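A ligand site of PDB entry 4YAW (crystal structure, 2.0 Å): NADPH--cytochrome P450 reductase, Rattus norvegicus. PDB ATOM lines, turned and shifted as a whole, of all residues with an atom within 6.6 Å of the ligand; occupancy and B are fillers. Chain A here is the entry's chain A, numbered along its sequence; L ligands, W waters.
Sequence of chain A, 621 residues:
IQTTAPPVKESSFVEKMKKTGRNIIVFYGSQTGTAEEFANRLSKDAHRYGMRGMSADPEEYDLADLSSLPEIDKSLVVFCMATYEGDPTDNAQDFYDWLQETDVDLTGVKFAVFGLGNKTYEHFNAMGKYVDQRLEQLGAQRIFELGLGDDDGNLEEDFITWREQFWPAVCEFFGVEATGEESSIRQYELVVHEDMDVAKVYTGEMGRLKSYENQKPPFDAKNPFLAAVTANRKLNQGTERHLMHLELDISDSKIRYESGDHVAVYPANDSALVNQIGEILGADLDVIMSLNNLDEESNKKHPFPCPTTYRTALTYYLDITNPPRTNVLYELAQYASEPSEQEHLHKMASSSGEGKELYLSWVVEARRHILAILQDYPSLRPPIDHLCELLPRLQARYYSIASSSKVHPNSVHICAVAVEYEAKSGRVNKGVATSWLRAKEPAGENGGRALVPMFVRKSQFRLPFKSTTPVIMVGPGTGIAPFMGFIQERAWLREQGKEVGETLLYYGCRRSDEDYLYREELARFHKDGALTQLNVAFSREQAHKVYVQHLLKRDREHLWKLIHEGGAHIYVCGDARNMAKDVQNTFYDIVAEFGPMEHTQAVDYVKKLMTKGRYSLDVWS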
ATOM      1  N   ARG A 241      33.464   3.363 -24.655  1.00  0.00           N
ATOM      2  CA  ARG A 241      34.057   3.318 -25.988  1.00  0.00           C
ATOM      3  C   ARG A 241      33.380   4.338 -26.895  1.00  0.00           C
ATOM      4  O   ARG A 241      32.373   4.930 -26.552  1.00  0.00           O
ATOM      5  CB  ARG A 241      33.871   1.933 -26.615  1.00  0.00           C
ATOM      6  CG  ARG A 241      34.593   0.790 -25.926  1.00  0.00           C
ATOM      7  CD  ARG A 241      34.007  -0.531 -26.436  1.00  0.00           C
ATOM      8  NE  ARG A 241      32.625  -0.671 -26.000  1.00  0.00           N
ATOM      9  CZ  ARG A 241      31.760  -1.536 -26.511  1.00  0.00           C
ATOM     10  NH1 ARG A 241      32.126  -2.361 -27.486  1.00  0.00           N
ATOM     11  NH2 ARG A 241      30.516  -1.589 -26.024  1.00  0.00           N
ATOM     12  N   PRO A 476      28.631  -9.634 -34.931  1.00  0.00           N
ATOM     13  CA  PRO A 476      28.536  -8.917 -33.662  1.00  0.00           C
ATOM     14  C   PRO A 476      29.458  -7.680 -33.622  1.00  0.00           C
ATOM     15  O   PRO A 476      30.447  -7.600 -34.362  1.00  0.00           O
ATOM     16  CB  PRO A 476      28.904  -9.992 -32.634  1.00  0.00           C
ATOM     17  CG  PRO A 476      29.850 -10.861 -33.378  1.00  0.00           C
ATOM     18  CD  PRO A 476      29.217 -10.978 -34.748  1.00  0.00           C
ATOM     19  N   GLY A 477      29.117  -6.713 -32.775  1.00  0.00           N
ATOM     20  CA  GLY A 477      29.912  -5.501 -32.697  1.00  0.00           C
ATOM     21  C   GLY A 477      29.987  -4.781 -34.033  1.00  0.00           C
ATOM     22  O   GLY A 477      28.989  -4.711 -34.765  1.00  0.00           O
ATOM     23  N   THR A 478      31.158  -4.256 -34.377  1.00  0.00           N
ATOM     24  CA  THR A 478      31.338  -3.552 -35.634  1.00  0.00           C
ATOM     25  C   THR A 478      31.238  -4.524 -36.823  1.00  0.00           C
ATOM     26  O   THR A 478      31.312  -4.109 -37.989  1.00  0.00           O
ATOM     27  CB  THR A 478      32.688  -2.815 -35.671  1.00  0.00           C
ATOM     28  OG1 THR A 478      33.760  -3.761 -35.538  1.00  0.00           O
ATOM     29  CG2 THR A 478      32.772  -1.799 -34.546  1.00  0.00           C
ATOM     30  N   GLY A 508      25.249  -8.954 -32.140  1.00  0.00           N
ATOM     31  CA  GLY A 508      25.550  -9.017 -30.731  1.00  0.00           C
ATOM     32  C   GLY A 508      26.246  -7.766 -30.205  1.00  0.00           C
ATOM     33  O   GLY A 508      27.032  -7.137 -30.914  1.00  0.00           O
ATOM     34  N   CYS A 509      25.938  -7.421 -28.965  1.00  0.00           N
ATOM     35  CA  CYS A 509      26.551  -6.281 -28.305  1.00  0.00           C
ATOM     36  C   CYS A 509      26.473  -6.537 -26.813  1.00  0.00           C
ATOM     37  O   CYS A 509      25.926  -7.553 -26.385  1.00  0.00           O
ATOM     38  CB  CYS A 509      25.831  -4.974 -28.676  1.00  0.00           C
ATOM     39  SG  CYS A 509      24.102  -4.840 -28.185  1.00  0.00           S
ATOM     40  N   ARG A 510      27.026  -5.643 -26.011  1.00  0.00           N
ATOM     41  CA  ARG A 510      27.004  -5.828 -24.564  1.00  0.00           C
ATOM     42  C   ARG A 510      25.617  -5.647 -23.948  1.00  0.00           C
ATOM     43  O   ARG A 510      25.103  -6.543 -23.285  1.00  0.00           O
ATOM     44  CB  ARG A 510      27.984  -4.862 -23.906  1.00  0.00           C
ATOM     45  CG  ARG A 510      29.417  -5.031 -24.400  1.00  0.00           C
ATOM     46  CD  ARG A 510      30.335  -4.051 -23.720  1.00  0.00           C
ATOM     47  NE  ARG A 510      31.716  -4.161 -24.187  1.00  0.00           N
ATOM     48  CZ  ARG A 510      32.697  -3.362 -23.783  1.00  0.00           C
ATOM     49  NH1 ARG A 510      32.447  -2.391 -22.905  1.00  0.00           N
ATOM     50  NH2 ARG A 510      33.911  -3.536 -24.254  1.00  0.00           N
ATOM     51  N   ARG A 511      25.002  -4.484 -24.181  1.00  0.00           N
ATOM     52  CA  ARG A 511      23.689  -4.179 -23.634  1.00  0.00           C
ATOM     53  C   ARG A 511      22.844  -3.346 -24.587  1.00  0.00           C
ATOM     54  O   ARG A 511      23.338  -2.429 -25.226  1.00  0.00           O
ATOM     55  CB  ARG A 511      23.817  -3.436 -22.296  1.00  0.00           C
ATOM     56  CG  ARG A 511      24.577  -4.169 -21.213  1.00  0.00           C
ATOM     57  CD  ARG A 511      24.324  -3.501 -19.872  1.00  0.00           C
ATOM     58  NE  ARG A 511      24.863  -4.266 -18.745  1.00  0.00           N
ATOM     59  CZ  ARG A 511      26.147  -4.348 -18.450  1.00  0.00           C
ATOM     60  NH1 ARG A 511      27.045  -3.708 -19.188  1.00  0.00           N
ATOM     61  NH2 ARG A 511      26.545  -5.074 -17.411  1.00  0.00           N
ATOM     62  N   ASP A 515      25.363  -0.174 -26.344  1.00  0.00           N
ATOM     63  CA  ASP A 515      26.100  -0.254 -27.611  1.00  0.00           C
ATOM     64  C   ASP A 515      25.388  -1.044 -28.707  1.00  0.00           C
ATOM     65  O   ASP A 515      26.019  -1.746 -29.498  1.00  0.00           O
ATOM     66  CB  ASP A 515      27.479  -0.864 -27.361  1.00  0.00           C
ATOM     67  CG  ASP A 515      27.398  -2.235 -26.718  1.00  0.00           C
ATOM     68  OD1 ASP A 515      26.309  -2.609 -26.245  1.00  0.00           O
ATOM     69  OD2 ASP A 515      28.432  -2.939 -26.671  1.00  0.00           O
ATOM     70  N   ALA A 537      22.184 -10.883 -29.421  1.00  0.00           N
ATOM     71  CA  ALA A 537      22.717 -11.434 -28.197  1.00  0.00           C
ATOM     72  C   ALA A 537      23.322 -10.301 -27.379  1.00  0.00           C
ATOM     73  O   ALA A 537      24.284  -9.661 -27.811  1.00  0.00           O
ATOM     74  CB  ALA A 537      23.792 -12.493 -28.505  1.00  0.00           C
ATOM     75  N   PHE A 538      22.737 -10.020 -26.222  1.00  0.00           N
ATOM     76  CA  PHE A 538      23.244  -8.979 -25.332  1.00  0.00           C
ATOM     77  C   PHE A 538      24.118  -9.742 -24.363  1.00  0.00           C
ATOM     78  O   PHE A 538      23.640 -10.335 -23.389  1.00  0.00           O
ATOM     79  CB  PHE A 538      22.085  -8.282 -24.613  1.00  0.00           C
ATOM     80  CG  PHE A 538      21.104  -7.617 -25.544  1.00  0.00           C
ATOM     81  CD1 PHE A 538      21.499  -6.559 -26.359  1.00  0.00           C
ATOM     82  CD2 PHE A 538      19.802  -8.093 -25.648  1.00  0.00           C
ATOM     83  CE1 PHE A 538      20.605  -5.969 -27.265  1.00  0.00           C
ATOM     84  CE2 PHE A 538      18.892  -7.514 -26.544  1.00  0.00           C
ATOM     85  CZ  PHE A 538      19.304  -6.456 -27.361  1.00  0.00           C
ATOM     86  N   SER A 539      25.413  -9.742 -24.656  1.00  0.00           N
ATOM     87  CA  SER A 539      26.399 -10.478 -23.888  1.00  0.00           C
ATOM     88  C   SER A 539      26.523 -10.167 -22.398  1.00  0.00           C
ATOM     89  O   SER A 539      26.958 -11.030 -21.640  1.00  0.00           O
ATOM     90  CB  SER A 539      27.777 -10.300 -24.524  1.00  0.00           C
ATOM     91  OG  SER A 539      28.228  -8.965 -24.367  1.00  0.00           O
ATOM     92  N   ARG A 540      26.122  -8.971 -21.975  1.00  0.00           N
ATOM     93  CA  ARG A 540      26.278  -8.602 -20.576  1.00  0.00           C
ATOM     94  C   ARG A 540      25.017  -8.303 -19.772  1.00  0.00           C
ATOM     95  O   ARG A 540      25.102  -7.802 -18.652  1.00  0.00           O
ATOM     96  CB  ARG A 540      27.228  -7.400 -20.476  1.00  0.00           C
ATOM     97  CG  ARG A 540      28.504  -7.600 -21.269  1.00  0.00           C
ATOM     98  CD  ARG A 540      29.559  -6.563 -20.951  1.00  0.00           C
ATOM     99  NE  ARG A 540      30.777  -6.809 -21.714  1.00  0.00           N
ATOM    100  CZ  ARG A 540      31.929  -6.179 -21.515  1.00  0.00           C
ATOM    101  NH1 ARG A 540      32.017  -5.259 -20.567  1.00  0.00           N
ATOM    102  NH2 ARG A 540      32.994  -6.468 -22.265  1.00  0.00           N
ATOM    103  N   LYS A 545      27.526 -15.295 -20.500  1.00  0.00           N
ATOM    104  CA  LYS A 545      27.777 -14.564 -21.739  1.00  0.00           C
ATOM    105  C   LYS A 545      26.775 -15.167 -22.729  1.00  0.00           C
ATOM    106  O   LYS A 545      26.613 -16.391 -22.784  1.00  0.00           O
ATOM    107  CB  LYS A 545      29.190 -14.845 -22.278  1.00  0.00           C
ATOM    108  CG  LYS A 545      30.332 -14.178 -21.529  1.00  0.00           C
ATOM    109  CD  LYS A 545      30.267 -12.662 -21.606  1.00  0.00           C
ATOM    110  CE  LYS A 545      31.514 -12.018 -20.999  1.00  0.00           C
ATOM    111  NZ  LYS A 545      31.373 -10.538 -20.873  1.00  0.00           N
ATOM    112  N   VAL A 546      26.085 -14.321 -23.481  1.00  0.00           N
ATOM    113  CA  VAL A 546      25.171 -14.791 -24.513  1.00  0.00           C
ATOM    114  C   VAL A 546      25.750 -14.186 -25.779  1.00  0.00           C
ATOM    115  O   VAL A 546      25.834 -12.967 -25.913  1.00  0.00           O
ATOM    116  CB  VAL A 546      23.713 -14.304 -24.301  1.00  0.00           C
ATOM    117  CG1 VAL A 546      22.841 -14.729 -25.490  1.00  0.00           C
ATOM    118  CG2 VAL A 546      23.139 -14.904 -23.043  1.00  0.00           C
ATOM    119  N   TYR A 547      26.196 -15.044 -26.685  1.00  0.00           N
ATOM    120  CA  TYR A 547      26.801 -14.634 -27.936  1.00  0.00           C
ATOM    121  C   TYR A 547      25.979 -15.095 -29.152  1.00  0.00           C
ATOM    122  O   TYR A 547      25.082 -15.912 -29.018  1.00  0.00           O
ATOM    123  CB  TYR A 547      28.210 -15.216 -28.062  1.00  0.00           C
ATOM    124  CG  TYR A 547      29.197 -14.755 -27.003  1.00  0.00           C
ATOM    125  CD1 TYR A 547      29.213 -13.421 -26.567  1.00  0.00           C
ATOM    126  CD2 TYR A 547      30.194 -15.610 -26.534  1.00  0.00           C
ATOM    127  CE1 TYR A 547      30.200 -12.958 -25.687  1.00  0.00           C
ATOM    128  CE2 TYR A 547      31.193 -15.151 -25.649  1.00  0.00           C
ATOM    129  CZ  TYR A 547      31.188 -13.830 -25.245  1.00  0.00           C
ATOM    130  OH  TYR A 547      32.189 -13.352 -24.424  1.00  0.00           O
ATOM    131  N   VAL A 548      26.317 -14.580 -30.327  1.00  0.00           N
ATOM    132  CA  VAL A 548      25.598 -14.951 -31.537  1.00  0.00           C
ATOM    133  C   VAL A 548      25.586 -16.462 -31.771  1.00  0.00           C
ATOM    134  O   VAL A 548      24.579 -17.013 -32.212  1.00  0.00           O
ATOM    135  CB  VAL A 548      26.192 -14.235 -32.786  1.00  0.00           C
ATOM    136  CG1 VAL A 548      25.933 -12.728 -32.702  1.00  0.00           C
ATOM    137  CG2 VAL A 548      27.686 -14.503 -32.886  1.00  0.00           C
ATOM    138  N   GLN A 549      26.699 -17.152 -31.477  1.00  0.00           N
ATOM    139  CA  GLN A 549      26.735 -18.591 -31.683  1.00  0.00           C
ATOM    140  C   GLN A 549      25.704 -19.317 -30.826  1.00  0.00           C
ATOM    141  O   GLN A 549      25.232 -20.386 -31.200  1.00  0.00           O
ATOM    142  CB  GLN A 549      28.141 -19.184 -31.395  1.00  0.00           C
ATOM    143  CG  GLN A 549      28.714 -18.861 -30.029  1.00  0.00           C
ATOM    144  CD  GLN A 549      29.595 -17.636 -30.083  1.00  0.00           C
ATOM    145  OE1 GLN A 549      29.242 -16.644 -30.712  1.00  0.00           O
ATOM    146  NE2 GLN A 549      30.742 -17.689 -29.407  1.00  0.00           N
ATOM    147  N   ASP A 575      35.330 -10.095 -35.476  1.00  0.00           N
ATOM    148  CA  ASP A 575      36.515 -10.679 -34.880  1.00  0.00           C
ATOM    149  C   ASP A 575      36.857 -12.043 -35.478  1.00  0.00           C
ATOM    150  O   ASP A 575      36.068 -12.987 -35.398  1.00  0.00           O
ATOM    151  CB  ASP A 575      36.324 -10.808 -33.376  1.00  0.00           C
ATOM    152  CG  ASP A 575      37.440 -11.587 -32.731  1.00  0.00           C
ATOM    153  OD1 ASP A 575      38.610 -11.268 -33.007  1.00  0.00           O
ATOM    154  OD2 ASP A 575      37.133 -12.523 -31.966  1.00  0.00           O
ATOM    155  N   ASN A 578      38.512 -15.084 -32.151  1.00  0.00           N
ATOM    156  CA  ASN A 578      37.692 -16.053 -31.438  1.00  0.00           C
ATOM    157  C   ASN A 578      36.248 -16.217 -31.907  1.00  0.00           C
ATOM    158  O   ASN A 578      35.755 -17.336 -32.013  1.00  0.00           O
ATOM    159  CB  ASN A 578      37.723 -15.761 -29.950  1.00  0.00           C
ATOM    160  CG  ASN A 578      39.116 -15.872 -29.362  1.00  0.00           C
ATOM    161  OD1 ASN A 578      39.951 -14.989 -29.511  1.00  0.00           O
ATOM    162  ND2 ASN A 578      39.385 -16.993 -28.699  1.00  0.00           N
ATOM    163  N   MET A 579      35.559 -15.107 -32.186  1.00  0.00           N
ATOM    164  CA  MET A 579      34.174 -15.177 -32.622  1.00  0.00           C
ATOM    165  C   MET A 579      33.999 -16.011 -33.895  1.00  0.00           C
ATOM    166  O   MET A 579      33.182 -16.929 -33.933  1.00  0.00           O
ATOM    167  CB  MET A 579      33.605 -13.768 -32.837  1.00  0.00           C
ATOM    168  CG  MET A 579      32.151 -13.711 -33.323  1.00  0.00           C
ATOM    169  SD  MET A 579      31.936 -14.018 -35.108  1.00  0.00           S
ATOM    170  CE  MET A 579      32.668 -12.550 -35.825  1.00  0.00           C
ATOM    171  N   ALA A 580      34.758 -15.690 -34.937  1.00  0.00           N
ATOM    172  CA  ALA A 580      34.672 -16.406 -36.210  1.00  0.00           C
ATOM    173  C   ALA A 580      34.840 -17.926 -36.061  1.00  0.00           C
ATOM    174  O   ALA A 580      34.114 -18.701 -36.684  1.00  0.00           O
ATOM    175  CB  ALA A 580      35.710 -15.866 -37.200  1.00  0.00           C
ATOM    176  N   ASP A 582      34.448 -19.714 -33.192  1.00  0.00           N
ATOM    177  CA  ASP A 582      33.362 -20.226 -32.382  1.00  0.00           C
ATOM    178  C   ASP A 582      32.101 -20.384 -33.225  1.00  0.00           C
ATOM    179  O   ASP A 582      31.357 -21.349 -33.079  1.00  0.00           O
ATOM    180  CB  ASP A 582      33.067 -19.314 -31.204  1.00  0.00           C
ATOM    181  CG  ASP A 582      34.166 -19.319 -30.173  1.00  0.00           C
ATOM    182  OD1 ASP A 582      34.926 -20.307 -30.119  1.00  0.00           O
ATOM    183  OD2 ASP A 582      34.261 -18.341 -29.419  1.00  0.00           O
ATOM    184  N   VAL A 583      31.868 -19.420 -34.104  1.00  0.00           N
ATOM    185  CA  VAL A 583      30.699 -19.493 -34.975  1.00  0.00           C
ATOM    186  C   VAL A 583      30.870 -20.668 -35.931  1.00  0.00           C
ATOM    187  O   VAL A 583      29.927 -21.414 -36.170  1.00  0.00           O
ATOM    188  CB  VAL A 583      30.515 -18.183 -35.781  1.00  0.00           C
ATOM    189  CG1 VAL A 583      29.541 -18.412 -36.939  1.00  0.00           C
ATOM    190  CG2 VAL A 583      30.004 -17.087 -34.864  1.00  0.00           C
HETATM  191  P1  LIG L   1      31.702  -9.448 -24.405  1.00  0.00           P
HETATM  192  O1  LIG L   1      30.733  -9.203 -23.304  1.00  0.00           O
HETATM  193  O2  LIG L   1      32.454 -10.712 -24.260  1.00  0.00           O
HETATM  194  O3  LIG L   1      32.539  -8.281 -24.760  1.00  0.00           O
HETATM  195  C1  LIG L   1      30.936  -7.148 -29.655  1.00  0.00           C
HETATM  196  O4  LIG L   1      32.236  -6.964 -29.082  1.00  0.00           O
HETATM  197  C2  LIG L   1      30.236  -8.358 -29.026  1.00  0.00           C
HETATM  198  O5  LIG L   1      30.993  -9.563 -29.267  1.00  0.00           O
HETATM  199  C3  LIG L   1      30.147  -8.198 -27.511  1.00  0.00           C
HETATM  200  O6  LIG L   1      28.816  -8.512 -27.086  1.00  0.00           O
HETATM  201  C4  LIG L   1      31.127  -9.244 -27.001  1.00  0.00           C
HETATM  202  O7  LIG L   1      30.758  -9.681 -25.688  1.00  0.00           O
HETATM  203  C5  LIG L   1      30.897 -10.314 -28.049  1.00  0.00           C
HETATM  204  N1  LIG L   1      31.889 -11.412 -28.031  1.00  0.00           N
HETATM  205  C6  LIG L   1      33.031 -11.482 -27.354  1.00  0.00           C
HETATM  206  N2  LIG L   1      33.607 -12.644 -27.629  1.00  0.00           N
HETATM  207  C7  LIG L   1      32.825 -13.307 -28.469  1.00  0.00           C
HETATM  208  C8  LIG L   1      32.915 -14.528 -29.000  1.00  0.00           C
HETATM  209  N3  LIG L   1      33.987 -15.251 -28.672  1.00  0.00           N
HETATM  210  N4  LIG L   1      31.979 -15.021 -29.815  1.00  0.00           N
HETATM  211  C9  LIG L   1      30.874 -14.221 -30.147  1.00  0.00           C
HETATM  212  N5  LIG L   1      30.801 -12.954 -29.569  1.00  0.00           N
HETATM  213  C10 LIG L   1      31.776 -12.533 -28.744  1.00  0.00           C
HETATM  214  O   HOH W   1      32.860 -10.559 -31.615  1.00  0.00           O
HETATM  215  O   HOH W   2      28.116 -12.248 -30.018  1.00  0.00           O
HETATM  216  O   HOH W   3      32.526  -5.973 -26.200  1.00  0.00           O
HETATM  217  O   HOH W   4      36.976 -12.636 -27.099  1.00  0.00           O
HETATM  218  O   HOH W   5      34.782 -10.981 -22.923  1.00  0.00           O
HETATM  219  O   HOH W   6      29.521  -4.403 -28.514  1.00  0.00           O
HETATM  220  O   HOH W   7      27.043 -10.512 -27.983  1.00  0.00           O
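Merely in contact with the ligand: Pro 476 (3.99 Å), Gly 477 (3.6 Å), Gly 508 (3.9 Å), Arg 510 (3.5 Å), Asn 578 (3.98 Å) and Met 579 (3.5 Å).
Hydrophobic or aromatic side chains that line the ligand: Pro 476, Tyr 547 and Met 579.
The side-chain hydroxyl of Tyr 547 is in hydrogen-bond range of an oxygen (O2) of the ligand, at 2.7 Å.
An oxygen (O1) of the ligand is in hydrogen-bond range of the side-chain hydroxyl (OG) of Ser 539 (2.7 Å).
NZ of Lys 545 lies within salt-bridge range of O1 of the ligand (2.8 Å).
The guanidinium group (NE) of Arg 540 is in salt-bridge range of an oxygen (O1) of the ligand (2.9 Å).
The side-chain amide nitrogen (NE2) of Gln 549 sits at hydrogen-bond distance from a nitrogen (N4) of the ligand, 3.0 Å away.
O of Cys 509 lies close to O6 of the ligand, 3.1 Å away.
A nitrogen (N3) of the ligand lies within hydrogen-bond range of the side-chain carboxylate (OD2) of Asp 582.
N of Ser 539 lies within hydrogen-bond range of O of Cys 509 (2.8 Å).
The backbone carbonyl oxygen of Arg 510 lies within hydrogen-bond range of the backbone NH of Arg 540, 2.9 Å away.
The backbone carbonyl oxygen (O) of Arg 540 sits at hydrogen-bond distance from the guanidinium group (NH2) of Arg 511 (3.3 Å).
The backbone carbonyl oxygen (O) of Ala 537 sits at hydrogen-bond distance from the backbone NH (N) of Cys 509, 3.0 Å away.
SG of Cys 509 sits close to OD1 of Asp 515 (3.7 Å).
OD2 of Asp 575 is in hydrogen-bond range of N of Met 579, at 3.0 Å.
N of Arg 510 is in hydrogen-bond range of OD2 of Asp 515, 3.1 Å away.
N of Gly 477 lies within hydrogen-bond range of O of Gly 508 (2.8 Å).
Water W3 lies within hydrogen-bond range of an oxygen (O3) of the ligand (2.7 Å) and the guanidinium group of Arg 510 (2.8 Å).
Water W2 bridges N5 of the ligand (2.8 Å) and N of Val 548 (3.0 Å).
Water W7 lies within hydrogen-bond range of O6 of the ligand (2.8 Å), O of Ala 537 (2.9 Å), N of Cys 509 (3.4 Å) and O of Val 546 (3.4 Å).
Water W6 bridges the side-chain carboxylate of Asp 515 (2.6 Å) and the guanidinium group of Arg 241 (3.5 Å).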
